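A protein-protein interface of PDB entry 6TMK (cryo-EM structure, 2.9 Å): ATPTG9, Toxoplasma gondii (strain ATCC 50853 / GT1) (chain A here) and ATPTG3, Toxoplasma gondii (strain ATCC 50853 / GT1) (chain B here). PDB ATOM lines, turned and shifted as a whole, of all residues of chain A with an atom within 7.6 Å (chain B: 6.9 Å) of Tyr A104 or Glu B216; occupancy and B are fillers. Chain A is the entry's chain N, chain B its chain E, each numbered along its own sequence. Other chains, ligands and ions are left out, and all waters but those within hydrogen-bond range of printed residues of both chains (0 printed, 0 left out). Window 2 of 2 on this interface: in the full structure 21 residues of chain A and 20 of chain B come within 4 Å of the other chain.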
ATOM      1  N   PRO A  71      23.844  -0.022 -14.043  1.00  0.00           N
ATOM      2  CA  PRO A  71      22.542  -0.647 -13.773  1.00  0.00           C
ATOM      3  C   PRO A  71      22.520  -1.447 -12.487  1.00  0.00           C
ATOM      4  O   PRO A  71      21.441  -1.670 -11.929  1.00  0.00           O
ATOM      5  CB  PRO A  71      22.337  -1.543 -14.998  1.00  0.00           C
ATOM      6  CG  PRO A  71      23.047  -0.831 -16.073  1.00  0.00           C
ATOM      7  CD  PRO A  71      24.292  -0.312 -15.414  1.00  0.00           C
ATOM      8  N   SER A  72      23.679  -1.892 -12.003  1.00  0.00           N
ATOM      9  CA  SER A  72      23.776  -2.492 -10.682  1.00  0.00           C
ATOM     10  C   SER A  72      23.608  -1.468  -9.570  1.00  0.00           C
ATOM     11  O   SER A  72      23.454  -1.858  -8.409  1.00  0.00           O
ATOM     12  CB  SER A  72      25.118  -3.205 -10.537  1.00  0.00           C
ATOM     13  OG  SER A  72      25.255  -3.792  -9.257  1.00  0.00           O
ATOM     14  N   PHE A  73      23.620  -0.177  -9.901  1.00  0.00           N
ATOM     15  CA  PHE A  73      23.583   0.897  -8.911  1.00  0.00           C
ATOM     16  C   PHE A  73      24.731   0.784  -7.911  1.00  0.00           C
ATOM     17  O   PHE A  73      24.577   1.085  -6.726  1.00  0.00           O
ATOM     18  CB  PHE A  73      22.238   0.928  -8.190  1.00  0.00           C
ATOM     19  CG  PHE A  73      21.078   1.211  -9.091  1.00  0.00           C
ATOM     20  CD1 PHE A  73      20.904   2.462  -9.636  1.00  0.00           C
ATOM     21  CD2 PHE A  73      20.154   0.228  -9.386  1.00  0.00           C
ATOM     22  CE1 PHE A  73      19.841   2.728 -10.462  1.00  0.00           C
ATOM     23  CE2 PHE A  73      19.089   0.493 -10.212  1.00  0.00           C
ATOM     24  CZ  PHE A  73      18.933   1.745 -10.748  1.00  0.00           C
ATOM     25  N   CYS A  74      25.896   0.350  -8.392  1.00  0.00           N
ATOM     26  CA  CYS A  74      27.149   0.447  -7.648  1.00  0.00           C
ATOM     27  C   CYS A  74      27.148  -0.432  -6.404  1.00  0.00           C
ATOM     28  O   CYS A  74      27.825  -0.130  -5.416  1.00  0.00           O
ATOM     29  CB  CYS A  74      27.451   1.897  -7.269  1.00  0.00           C
ATOM     30  SG  CYS A  74      27.079   3.092  -8.560  1.00  0.00           S
ATOM     31  N   ALA A  75      26.405  -1.534  -6.453  1.00  0.00           N
ATOM     32  CA  ALA A  75      26.263  -2.388  -5.282  1.00  0.00           C
ATOM     33  C   ALA A  75      27.591  -3.021  -4.901  1.00  0.00           C
ATOM     34  O   ALA A  75      27.919  -3.135  -3.712  1.00  0.00           O
ATOM     35  CB  ALA A  75      25.215  -3.455  -5.564  1.00  0.00           C
ATOM     36  N   LYS A  76      28.361  -3.456  -5.897  1.00  0.00           N
ATOM     37  CA  LYS A  76      29.641  -4.088  -5.620  1.00  0.00           C
ATOM     38  C   LYS A  76      30.619  -3.090  -5.020  1.00  0.00           C
ATOM     39  O   LYS A  76      31.382  -3.431  -4.112  1.00  0.00           O
ATOM     40  CB  LYS A  76      30.194  -4.704  -6.898  1.00  0.00           C
ATOM     41  CG  LYS A  76      29.425  -5.937  -7.331  1.00  0.00           C
ATOM     42  CD  LYS A  76      29.905  -6.485  -8.656  1.00  0.00           C
ATOM     43  CE  LYS A  76      28.871  -7.421  -9.253  1.00  0.00           C
ATOM     44  NZ  LYS A  76      29.397  -8.186 -10.415  1.00  0.00           N
ATOM     45  N   GLU A  77      30.577  -1.841  -5.483  1.00  0.00           N
ATOM     46  CA  GLU A  77      31.389  -0.794  -4.876  1.00  0.00           C
ATOM     47  C   GLU A  77      30.987  -0.558  -3.428  1.00  0.00           C
ATOM     48  O   GLU A  77      31.845  -0.416  -2.547  1.00  0.00           O
ATOM     49  CB  GLU A  77      31.252   0.492  -5.685  1.00  0.00           C
ATOM     50  CG  GLU A  77      32.077   0.526  -6.951  1.00  0.00           C
ATOM     51  CD  GLU A  77      31.514  -0.357  -8.042  1.00  0.00           C
ATOM     52  OE1 GLU A  77      30.277  -0.398  -8.196  1.00  0.00           O
ATOM     53  OE2 GLU A  77      32.308  -1.011  -8.750  1.00  0.00           O
ATOM     54  N   VAL A  79      29.484  -2.644  -1.263  1.00  0.00           N
ATOM     55  CA  VAL A  79      29.884  -3.744  -0.396  1.00  0.00           C
ATOM     56  C   VAL A  79      31.400  -3.815  -0.271  1.00  0.00           C
ATOM     57  O   VAL A  79      31.922  -4.167   0.793  1.00  0.00           O
ATOM     58  CB  VAL A  79      29.286  -5.065  -0.911  1.00  0.00           C
ATOM     59  CG1 VAL A  79      29.902  -5.449  -2.211  1.00  0.00           C
ATOM     60  CG2 VAL A  79      29.500  -6.169   0.089  1.00  0.00           C
ATOM     61  N   ALA A  80      32.134  -3.463  -1.328  1.00  0.00           N
ATOM     62  CA  ALA A  80      33.588  -3.449  -1.241  1.00  0.00           C
ATOM     63  C   ALA A  80      34.070  -2.430  -0.223  1.00  0.00           C
ATOM     64  O   ALA A  80      34.961  -2.717   0.582  1.00  0.00           O
ATOM     65  CB  ALA A  80      34.185  -3.148  -2.610  1.00  0.00           C
ATOM     66  N   LEU A  92      33.692 -10.742   3.736  1.00  0.00           N
ATOM     67  CA  LEU A  92      33.099 -11.153   2.474  1.00  0.00           C
ATOM     68  C   LEU A  92      33.851 -10.480   1.339  1.00  0.00           C
ATOM     69  O   LEU A  92      34.096  -9.270   1.385  1.00  0.00           O
ATOM     70  CB  LEU A  92      31.619 -10.779   2.434  1.00  0.00           C
ATOM     71  CG  LEU A  92      30.819 -11.222   1.218  1.00  0.00           C
ATOM     72  CD1 LEU A  92      30.475 -12.680   1.334  1.00  0.00           C
ATOM     73  CD2 LEU A  92      29.565 -10.394   1.098  1.00  0.00           C
ATOM     74  N   VAL A  93      34.211 -11.257   0.321  1.00  0.00           N
ATOM     75  CA  VAL A  93      34.924 -10.746  -0.837  1.00  0.00           C
ATOM     76  C   VAL A  93      34.294 -11.308  -2.102  1.00  0.00           C
ATOM     77  O   VAL A  93      33.413 -12.166  -2.066  1.00  0.00           O
ATOM     78  CB  VAL A  93      36.426 -11.087  -0.792  1.00  0.00           C
ATOM     79  CG1 VAL A  93      37.014 -10.680   0.537  1.00  0.00           C
ATOM     80  CG2 VAL A  93      36.639 -12.565  -1.035  1.00  0.00           C
ATOM     81  N   LEU A  94      34.749 -10.782  -3.231  1.00  0.00           N
ATOM     82  CA  LEU A  94      34.304 -11.209  -4.548  1.00  0.00           C
ATOM     83  C   LEU A  94      35.425 -12.023  -5.177  1.00  0.00           C
ATOM     84  O   LEU A  94      36.525 -11.504  -5.397  1.00  0.00           O
ATOM     85  CB  LEU A  94      33.944 -10.005  -5.414  1.00  0.00           C
ATOM     86  CG  LEU A  94      33.116 -10.259  -6.668  1.00  0.00           C
ATOM     87  CD1 LEU A  94      31.790 -10.882  -6.319  1.00  0.00           C
ATOM     88  CD2 LEU A  94      32.900  -8.964  -7.409  1.00  0.00           C
ATOM     89  N   SER A  95      35.145 -13.289  -5.468  1.00  0.00           N
ATOM     90  CA  SER A  95      36.172 -14.189  -5.963  1.00  0.00           C
ATOM     91  C   SER A  95      36.652 -13.760  -7.339  1.00  0.00           C
ATOM     92  O   SER A  95      35.864 -13.329  -8.186  1.00  0.00           O
ATOM     93  CB  SER A  95      35.631 -15.615  -6.026  1.00  0.00           C
ATOM     94  OG  SER A  95      34.986 -15.853  -7.265  1.00  0.00           O
ATOM     95  N   PRO A 101      31.115 -16.242 -14.609  1.00  0.00           N
ATOM     96  CA  PRO A 101      30.354 -15.617 -13.538  1.00  0.00           C
ATOM     97  C   PRO A 101      31.177 -15.506 -12.267  1.00  0.00           C
ATOM     98  O   PRO A 101      31.774 -16.498 -11.818  1.00  0.00           O
ATOM     99  CB  PRO A 101      29.176 -16.579 -13.358  1.00  0.00           C
ATOM    100  CG  PRO A 101      29.770 -17.933 -13.682  1.00  0.00           C
ATOM    101  CD  PRO A 101      31.005 -17.708 -14.543  1.00  0.00           C
ATOM    102  N   PRO A 102      31.242 -14.327 -11.659  1.00  0.00           N
ATOM    103  CA  PRO A 102      31.913 -14.207 -10.366  1.00  0.00           C
ATOM    104  C   PRO A 102      31.017 -14.655  -9.222  1.00  0.00           C
ATOM    105  O   PRO A 102      29.791 -14.695  -9.326  1.00  0.00           O
ATOM    106  CB  PRO A 102      32.224 -12.712 -10.269  1.00  0.00           C
ATOM    107  CG  PRO A 102      31.154 -12.070 -11.050  1.00  0.00           C
ATOM    108  CD  PRO A 102      30.784 -13.018 -12.153  1.00  0.00           C
ATOM    109  N   HIS A 103      31.664 -14.996  -8.115  1.00  0.00           N
ATOM    110  CA  HIS A 103      30.993 -15.552  -6.954  1.00  0.00           C
ATOM    111  C   HIS A 103      31.329 -14.727  -5.723  1.00  0.00           C
ATOM    112  O   HIS A 103      32.373 -14.075  -5.660  1.00  0.00           O
ATOM    113  CB  HIS A 103      31.389 -17.012  -6.728  1.00  0.00           C
ATOM    114  CG  HIS A 103      30.612 -17.981  -7.559  1.00  0.00           C
ATOM    115  ND1 HIS A 103      30.138 -19.175  -7.063  1.00  0.00           N
ATOM    116  CD2 HIS A 103      30.223 -17.931  -8.854  1.00  0.00           C
ATOM    117  CE1 HIS A 103      29.493 -19.821  -8.018  1.00  0.00           C
ATOM    118  NE2 HIS A 103      29.529 -19.087  -9.115  1.00  0.00           N
ATOM    119  N   TYR A 104      30.418 -14.727  -4.758  1.00  0.00           N
ATOM    120  CA  TYR A 104      30.704 -14.154  -3.454  1.00  0.00           C
ATOM    121  C   TYR A 104      31.353 -15.232  -2.601  1.00  0.00           C
ATOM    122  O   TYR A 104      30.883 -16.373  -2.573  1.00  0.00           O
ATOM    123  CB  TYR A 104      29.437 -13.635  -2.778  1.00  0.00           C
ATOM    124  CG  TYR A 104      29.051 -12.227  -3.156  1.00  0.00           C
ATOM    125  CD1 TYR A 104      29.938 -11.179  -2.992  1.00  0.00           C
ATOM    126  CD2 TYR A 104      27.789 -11.942  -3.649  1.00  0.00           C
ATOM    127  CE1 TYR A 104      29.591  -9.893  -3.328  1.00  0.00           C
ATOM    128  CE2 TYR A 104      27.431 -10.657  -3.987  1.00  0.00           C
ATOM    129  CZ  TYR A 104      28.335  -9.636  -3.820  1.00  0.00           C
ATOM    130  OH  TYR A 104      27.983  -8.350  -4.156  1.00  0.00           O
ATOM    131  N   GLU A 105      32.425 -14.873  -1.907  1.00  0.00           N
ATOM    132  CA  GLU A 105      33.179 -15.817  -1.107  1.00  0.00           C
ATOM    133  C   GLU A 105      33.359 -15.267   0.296  1.00  0.00           C
ATOM    134  O   GLU A 105      33.405 -14.051   0.509  1.00  0.00           O
ATOM    135  CB  GLU A 105      34.546 -16.119  -1.723  1.00  0.00           C
ATOM    136  CG  GLU A 105      34.536 -17.277  -2.701  1.00  0.00           C
ATOM    137  CD  GLU A 105      35.924 -17.816  -2.985  1.00  0.00           C
ATOM    138  OE1 GLU A 105      36.686 -18.037  -2.021  1.00  0.00           O
ATOM    139  OE2 GLU A 105      36.250 -18.023  -4.173  1.00  0.00           O
ATOM    140  N   LEU A 106      33.450 -16.181   1.249  1.00  0.00           N
ATOM    141  CA  LEU A 106      33.604 -15.849   2.652  1.00  0.00           C
ATOM    142  C   LEU A 106      34.946 -16.370   3.140  1.00  0.00           C
ATOM    143  O   LEU A 106      35.338 -17.496   2.819  1.00  0.00           O
ATOM    144  CB  LEU A 106      32.465 -16.457   3.468  1.00  0.00           C
ATOM    145  CG  LEU A 106      32.305 -16.027   4.917  1.00  0.00           C
ATOM    146  CD1 LEU A 106      31.722 -14.638   5.001  1.00  0.00           C
ATOM    147  CD2 LEU A 106      31.418 -17.019   5.615  1.00  0.00           C
ATOM    148  N   THR A 119      32.191 -21.786   2.047  1.00  0.00           N
ATOM    149  CA  THR A 119      32.513 -20.380   1.851  1.00  0.00           C
ATOM    150  C   THR A 119      31.818 -19.766   0.645  1.00  0.00           C
ATOM    151  O   THR A 119      31.721 -18.537   0.567  1.00  0.00           O
ATOM    152  CB  THR A 119      34.024 -20.204   1.690  1.00  0.00           C
ATOM    153  OG1 THR A 119      34.489 -21.004   0.598  1.00  0.00           O
ATOM    154  CG2 THR A 119      34.742 -20.620   2.955  1.00  0.00           C
ATOM    155  N   ASP A 120      31.341 -20.580  -0.292  1.00  0.00           N
ATOM    156  CA  ASP A 120      30.709 -20.070  -1.504  1.00  0.00           C
ATOM    157  C   ASP A 120      29.263 -19.705  -1.196  1.00  0.00           C
ATOM    158  O   ASP A 120      28.432 -20.582  -0.943  1.00  0.00           O
ATOM    159  CB  ASP A 120      30.783 -21.108  -2.618  1.00  0.00           C
ATOM    160  CG  ASP A 120      30.557 -20.507  -3.991  1.00  0.00           C
ATOM    161  OD1 ASP A 120      30.451 -21.277  -4.969  1.00  0.00           O
ATOM    162  OD2 ASP A 120      30.482 -19.265  -4.095  1.00  0.00           O
ATOM    163  N   LEU A 121      28.962 -18.408  -1.217  1.00  0.00           N
ATOM    164  CA  LEU A 121      27.620 -17.904  -0.971  1.00  0.00           C
ATOM    165  C   LEU A 121      26.827 -17.690  -2.252  1.00  0.00           C
ATOM    166  O   LEU A 121      25.798 -17.008  -2.226  1.00  0.00           O
ATOM    167  CB  LEU A 121      27.691 -16.601  -0.180  1.00  0.00           C
ATOM    168  CG  LEU A 121      28.581 -16.648   1.053  1.00  0.00           C
ATOM    169  CD1 LEU A 121      28.537 -15.326   1.755  1.00  0.00           C
ATOM    170  CD2 LEU A 121      28.140 -17.757   1.982  1.00  0.00           C
ATOM    171  N   GLY A 122      27.281 -18.248  -3.363  1.00  0.00           N
ATOM    172  CA  GLY A 122      26.569 -18.156  -4.621  1.00  0.00           C
ATOM    173  C   GLY A 122      27.084 -17.038  -5.504  1.00  0.00           C
ATOM    174  O   GLY A 122      27.951 -16.241  -5.136  1.00  0.00           O
ATOM    175  N   SER A 123      26.512 -16.995  -6.702  1.00  0.00           N
ATOM    176  CA  SER A 123      26.926 -16.033  -7.709  1.00  0.00           C
ATOM    177  C   SER A 123      26.576 -14.610  -7.298  1.00  0.00           C
ATOM    178  O   SER A 123      25.648 -14.369  -6.522  1.00  0.00           O
ATOM    179  CB  SER A 123      26.270 -16.354  -9.047  1.00  0.00           C
ATOM    180  OG  SER A 123      26.249 -15.219  -9.886  1.00  0.00           O
ATOM    181  N   ALA A 124      27.334 -13.660  -7.838  1.00  0.00           N
ATOM    182  CA  ALA A 124      27.114 -12.247  -7.586  1.00  0.00           C
ATOM    183  C   ALA A 124      26.174 -11.610  -8.598  1.00  0.00           C
ATOM    184  O   ALA A 124      25.977 -10.392  -8.559  1.00  0.00           O
ATOM    185  CB  ALA A 124      28.449 -11.503  -7.589  1.00  0.00           C
ATOM    186  N   VAL A 125      25.600 -12.396  -9.502  1.00  0.00           N
ATOM    187  CA  VAL A 125      24.603 -11.923 -10.451  1.00  0.00           C
ATOM    188  C   VAL A 125      23.439 -12.898 -10.453  1.00  0.00           C
ATOM    189  O   VAL A 125      23.610 -14.102 -10.237  1.00  0.00           O
ATOM    190  CB  VAL A 125      25.176 -11.764 -11.874  1.00  0.00           C
ATOM    191  CG1 VAL A 125      26.410 -10.889 -11.852  1.00  0.00           C
ATOM    192  CG2 VAL A 125      25.494 -13.118 -12.473  1.00  0.00           C
ATOM    193  N   ALA A 126      22.246 -12.373 -10.707  1.00  0.00           N
ATOM    194  CA  ALA A 126      21.055 -13.192 -10.665  1.00  0.00           C
ATOM    195  C   ALA A 126      21.032 -14.160 -11.843  1.00  0.00           C
ATOM    196  O   ALA A 126      21.746 -13.971 -12.829  1.00  0.00           O
ATOM    197  CB  ALA A 126      19.812 -12.314 -10.686  1.00  0.00           C
ATOM    198  N   PRO B 212      15.347  -3.720 -11.408  1.00  0.00           N
ATOM    199  CA  PRO B 212      15.099  -3.764  -9.968  1.00  0.00           C
ATOM    200  C   PRO B 212      16.314  -4.272  -9.210  1.00  0.00           C
ATOM    201  O   PRO B 212      17.213  -4.909  -9.760  1.00  0.00           O
ATOM    202  CB  PRO B 212      13.919  -4.731  -9.840  1.00  0.00           C
ATOM    203  CG  PRO B 212      13.976  -5.558 -11.055  1.00  0.00           C
ATOM    204  CD  PRO B 212      14.516  -4.690 -12.135  1.00  0.00           C
ATOM    205  N   VAL B 213      16.324  -3.971  -7.912  1.00  0.00           N
ATOM    206  CA  VAL B 213      17.429  -4.379  -7.056  1.00  0.00           C
ATOM    207  C   VAL B 213      17.401  -5.859  -6.726  1.00  0.00           C
ATOM    208  O   VAL B 213      18.362  -6.371  -6.146  1.00  0.00           O
ATOM    209  CB  VAL B 213      17.413  -3.547  -5.761  1.00  0.00           C
ATOM    210  CG1 VAL B 213      17.359  -2.079  -6.087  1.00  0.00           C
ATOM    211  CG2 VAL B 213      16.231  -3.924  -4.906  1.00  0.00           C
ATOM    212  N   THR B 214      16.322  -6.554  -7.073  1.00  0.00           N
ATOM    213  CA  THR B 214      16.258  -7.992  -6.877  1.00  0.00           C
ATOM    214  C   THR B 214      17.226  -8.750  -7.772  1.00  0.00           C
ATOM    215  O   THR B 214      17.444  -9.943  -7.545  1.00  0.00           O
ATOM    216  CB  THR B 214      14.838  -8.487  -7.121  1.00  0.00           C
ATOM    217  OG1 THR B 214      14.445  -8.192  -8.467  1.00  0.00           O
ATOM    218  CG2 THR B 214      13.893  -7.813  -6.174  1.00  0.00           C
ATOM    219  N   THR B 215      17.802  -8.093  -8.777  1.00  0.00           N
ATOM    220  CA  THR B 215      18.855  -8.712  -9.567  1.00  0.00           C
ATOM    221  C   THR B 215      20.160  -8.801  -8.799  1.00  0.00           C
ATOM    222  O   THR B 215      21.041  -9.580  -9.179  1.00  0.00           O
ATOM    223  CB  THR B 215      19.079  -7.931 -10.858  1.00  0.00           C
ATOM    224  OG1 THR B 215      19.635  -6.647 -10.556  1.00  0.00           O
ATOM    225  CG2 THR B 215      17.778  -7.743 -11.580  1.00  0.00           C
ATOM    226  N   GLU B 216      20.301  -8.025  -7.731  1.00  0.00           N
ATOM    227  CA  GLU B 216      21.502  -8.035  -6.924  1.00  0.00           C
ATOM    228  C   GLU B 216      21.283  -8.946  -5.728  1.00  0.00           C
ATOM    229  O   GLU B 216      20.321  -8.734  -4.976  1.00  0.00           O
ATOM    230  CB  GLU B 216      21.853  -6.628  -6.465  1.00  0.00           C
ATOM    231  CG  GLU B 216      23.326  -6.422  -6.200  1.00  0.00           C
ATOM    232  CD  GLU B 216      23.695  -6.623  -4.754  1.00  0.00           C
ATOM    233  OE1 GLU B 216      22.974  -6.096  -3.883  1.00  0.00           O
ATOM    234  OE2 GLU B 216      24.706  -7.307  -4.489  1.00  0.00           O
ATOM    235  N   PRO B 217      22.120  -9.962  -5.510  1.00  0.00           N
ATOM    236  CA  PRO B 217      21.857 -10.887  -4.401  1.00  0.00           C
ATOM    237  C   PRO B 217      22.045 -10.265  -3.036  1.00  0.00           C
ATOM    238  O   PRO B 217      21.351 -10.660  -2.093  1.00  0.00           O
ATOM    239  CB  PRO B 217      22.855 -12.023  -4.648  1.00  0.00           C
ATOM    240  CG  PRO B 217      23.216 -11.903  -6.066  1.00  0.00           C
ATOM    241  CD  PRO B 217      23.212 -10.456  -6.357  1.00  0.00           C
ATOM    242  N   PHE B 218      22.963  -9.320  -2.890  1.00  0.00           N
ATOM    243  CA  PHE B 218      23.133  -8.666  -1.607  1.00  0.00           C
ATOM    244  C   PHE B 218      21.932  -7.776  -1.315  1.00  0.00           C
ATOM    245  O   PHE B 218      21.290  -7.238  -2.218  1.00  0.00           O
ATOM    246  CB  PHE B 218      24.421  -7.851  -1.587  1.00  0.00           C
ATOM    247  CG  PHE B 218      24.966  -7.627  -0.216  1.00  0.00           C
ATOM    248  CD1 PHE B 218      25.614  -8.639   0.462  1.00  0.00           C
ATOM    249  CD2 PHE B 218      24.822  -6.405   0.400  1.00  0.00           C
ATOM    250  CE1 PHE B 218      26.106  -8.430   1.724  1.00  0.00           C
ATOM    251  CE2 PHE B 218      25.310  -6.192   1.657  1.00  0.00           C
ATOM    252  CZ  PHE B 218      25.957  -7.204   2.323  1.00  0.00           C
ATOM    253  N   VAL B 219      21.635  -7.624  -0.030  1.00  0.00           N
ATOM    254  CA  VAL B 219      20.442  -6.936   0.441  1.00  0.00           C
ATOM    255  C   VAL B 219      20.882  -5.813   1.365  1.00  0.00           C
ATOM    256  O   VAL B 219      21.459  -6.065   2.430  1.00  0.00           O
ATOM    257  CB  VAL B 219      19.476  -7.895   1.154  1.00  0.00           C
ATOM    258  CG1 VAL B 219      18.349  -7.137   1.792  1.00  0.00           C
ATOM    259  CG2 VAL B 219      18.936  -8.923   0.193  1.00  0.00           C
ATOM    260  N   PHE B 220      20.610  -4.578   0.956  1.00  0.00           N
ATOM    261  CA  PHE B 220      20.925  -3.390   1.731  1.00  0.00           C
ATOM    262  C   PHE B 220      19.767  -2.924   2.598  1.00  0.00           C
ATOM    263  O   PHE B 220      19.896  -1.909   3.286  1.00  0.00           O
ATOM    264  CB  PHE B 220      21.328  -2.255   0.794  1.00  0.00           C
ATOM    265  CG  PHE B 220      22.443  -2.602  -0.136  1.00  0.00           C
ATOM    266  CD1 PHE B 220      23.740  -2.264   0.163  1.00  0.00           C
ATOM    267  CD2 PHE B 220      22.191  -3.254  -1.322  1.00  0.00           C
ATOM    268  CE1 PHE B 220      24.757  -2.576  -0.691  1.00  0.00           C
ATOM    269  CE2 PHE B 220      23.209  -3.563  -2.177  1.00  0.00           C
ATOM    270  CZ  PHE B 220      24.491  -3.228  -1.860  1.00  0.00           C
ATOM    271  N   ILE B 227      21.342 -12.446   2.021  1.00  0.00           N
ATOM    272  CA  ILE B 227      21.672 -12.836   0.658  1.00  0.00           C
ATOM    273  C   ILE B 227      20.431 -13.447   0.027  1.00  0.00           C
ATOM    274  O   ILE B 227      19.710 -14.209   0.675  1.00  0.00           O
ATOM    275  CB  ILE B 227      22.851 -13.829   0.612  1.00  0.00           C
ATOM    276  CG1 ILE B 227      24.167 -13.126   0.940  1.00  0.00           C
ATOM    277  CG2 ILE B 227      22.950 -14.470  -0.742  1.00  0.00           C
ATOM    278  CD1 ILE B 227      24.748 -12.339  -0.196  1.00  0.00           C
ATOM    279  N   ARG B 228      20.170 -13.103  -1.227  1.00  0.00           N
ATOM    280  CA  ARG B 228      18.989 -13.619  -1.899  1.00  0.00           C
ATOM    281  C   ARG B 228      19.227 -15.027  -2.420  1.00  0.00           C
ATOM    282  O   ARG B 228      20.279 -15.331  -2.989  1.00  0.00           O
ATOM    283  CB  ARG B 228      18.581 -12.714  -3.057  1.00  0.00           C
ATOM    284  CG  ARG B 228      18.134 -11.348  -2.642  1.00  0.00           C
ATOM    285  CD  ARG B 228      17.844 -10.482  -3.833  1.00  0.00           C
ATOM    286  NE  ARG B 228      17.563  -9.106  -3.458  1.00  0.00           N
ATOM    287  CZ  ARG B 228      16.430  -8.704  -2.904  1.00  0.00           C
ATOM    288  NH1 ARG B 228      15.462  -9.570  -2.658  1.00  0.00           N
ATOM    289  NH2 ARG B 228      16.264  -7.432  -2.598  1.00  0.00           N
ATOM    290  N   TYR B 230      17.538 -17.557  -5.110  1.00  0.00           N
ATOM    291  CA  TYR B 230      16.679 -17.472  -6.279  1.00  0.00           C
ATOM    292  C   TYR B 230      16.142 -18.848  -6.635  1.00  0.00           C
ATOM    293  O   TYR B 230      16.863 -19.846  -6.565  1.00  0.00           O
ATOM    294  CB  TYR B 230      17.431 -16.896  -7.477  1.00  0.00           C
ATOM    295  CG  TYR B 230      17.927 -15.487  -7.302  1.00  0.00           C
ATOM    296  CD1 TYR B 230      17.105 -14.410  -7.554  1.00  0.00           C
ATOM    297  CD2 TYR B 230      19.227 -15.235  -6.911  1.00  0.00           C
ATOM    298  CE1 TYR B 230      17.555 -13.126  -7.405  1.00  0.00           C
ATOM    299  CE2 TYR B 230      19.685 -13.954  -6.762  1.00  0.00           C
ATOM    300  CZ  TYR B 230      18.847 -12.903  -7.013  1.00  0.00           C
ATOM    301  OH  TYR B 230      19.291 -11.618  -6.866  1.00  0.00           O
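Among the printed residues, merely in contact across the chains: Ala A75 with Glu B216 (3.6 Å), Ala A75 with Phe B220 (3.8 Å), Ser A123 with Pro B217 (3.5 Å), Ala A124 with Pro B217 (3.5 Å) and Ala A126 with Tyr B230 (3.8 Å).
Of the 12 printed residues of chain B, 5 touch a printed residue of chain A.
Hydrophobic or aromatic side chains of chain B within 4 Å of the printed part of chain A: Pro B217, Phe B220 and Tyr B230.
Among the printed residues, 7 pairs touch across the chains.
O of Thr B215 sits close to N of Ala A126 (3.4 Å).
OH of Tyr A104 lies within hydrogen-bond range of OE2 of Glu B216, 3.5 Å away.
O of Pro B212 sits at hydrogen-bond distance from OG1 of Thr B215 (3.1 Å).
The backbone carbonyl oxygen of Thr B214 is in hydrogen-bond range of the side-chain hydroxyl of Tyr B230 (2.6 Å).
The side-chain carboxylate (OE2) of Glu B216 lies close to the backbone NH (N) of Phe B218, 3.1 Å away.
NE of Arg B228 is in hydrogen-bond range of O of Glu B216, 3.2 Å away.
O of Tyr A104 is in hydrogen-bond range of N of Leu A121 (3.1 Å).
O of Val A125 sits at hydrogen-bond distance from OG of Ser A123 (2.9 Å).
Tyr A104 touches just one residue of chain B: Glu B216 (3.5 Å).
Of the printed residues of chain B, Ala A124 touches Pro B217 (3.5 Å).
Of the printed residues of chain A, Glu B216 touches Ala A75 and Tyr A104.
Of the printed residues of chain A, Tyr B230 touches Ala A126 (3.8 Å).
The nearest printed residue of chain A that does not touch Phe B220 is Val A79 (4.8 Å).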
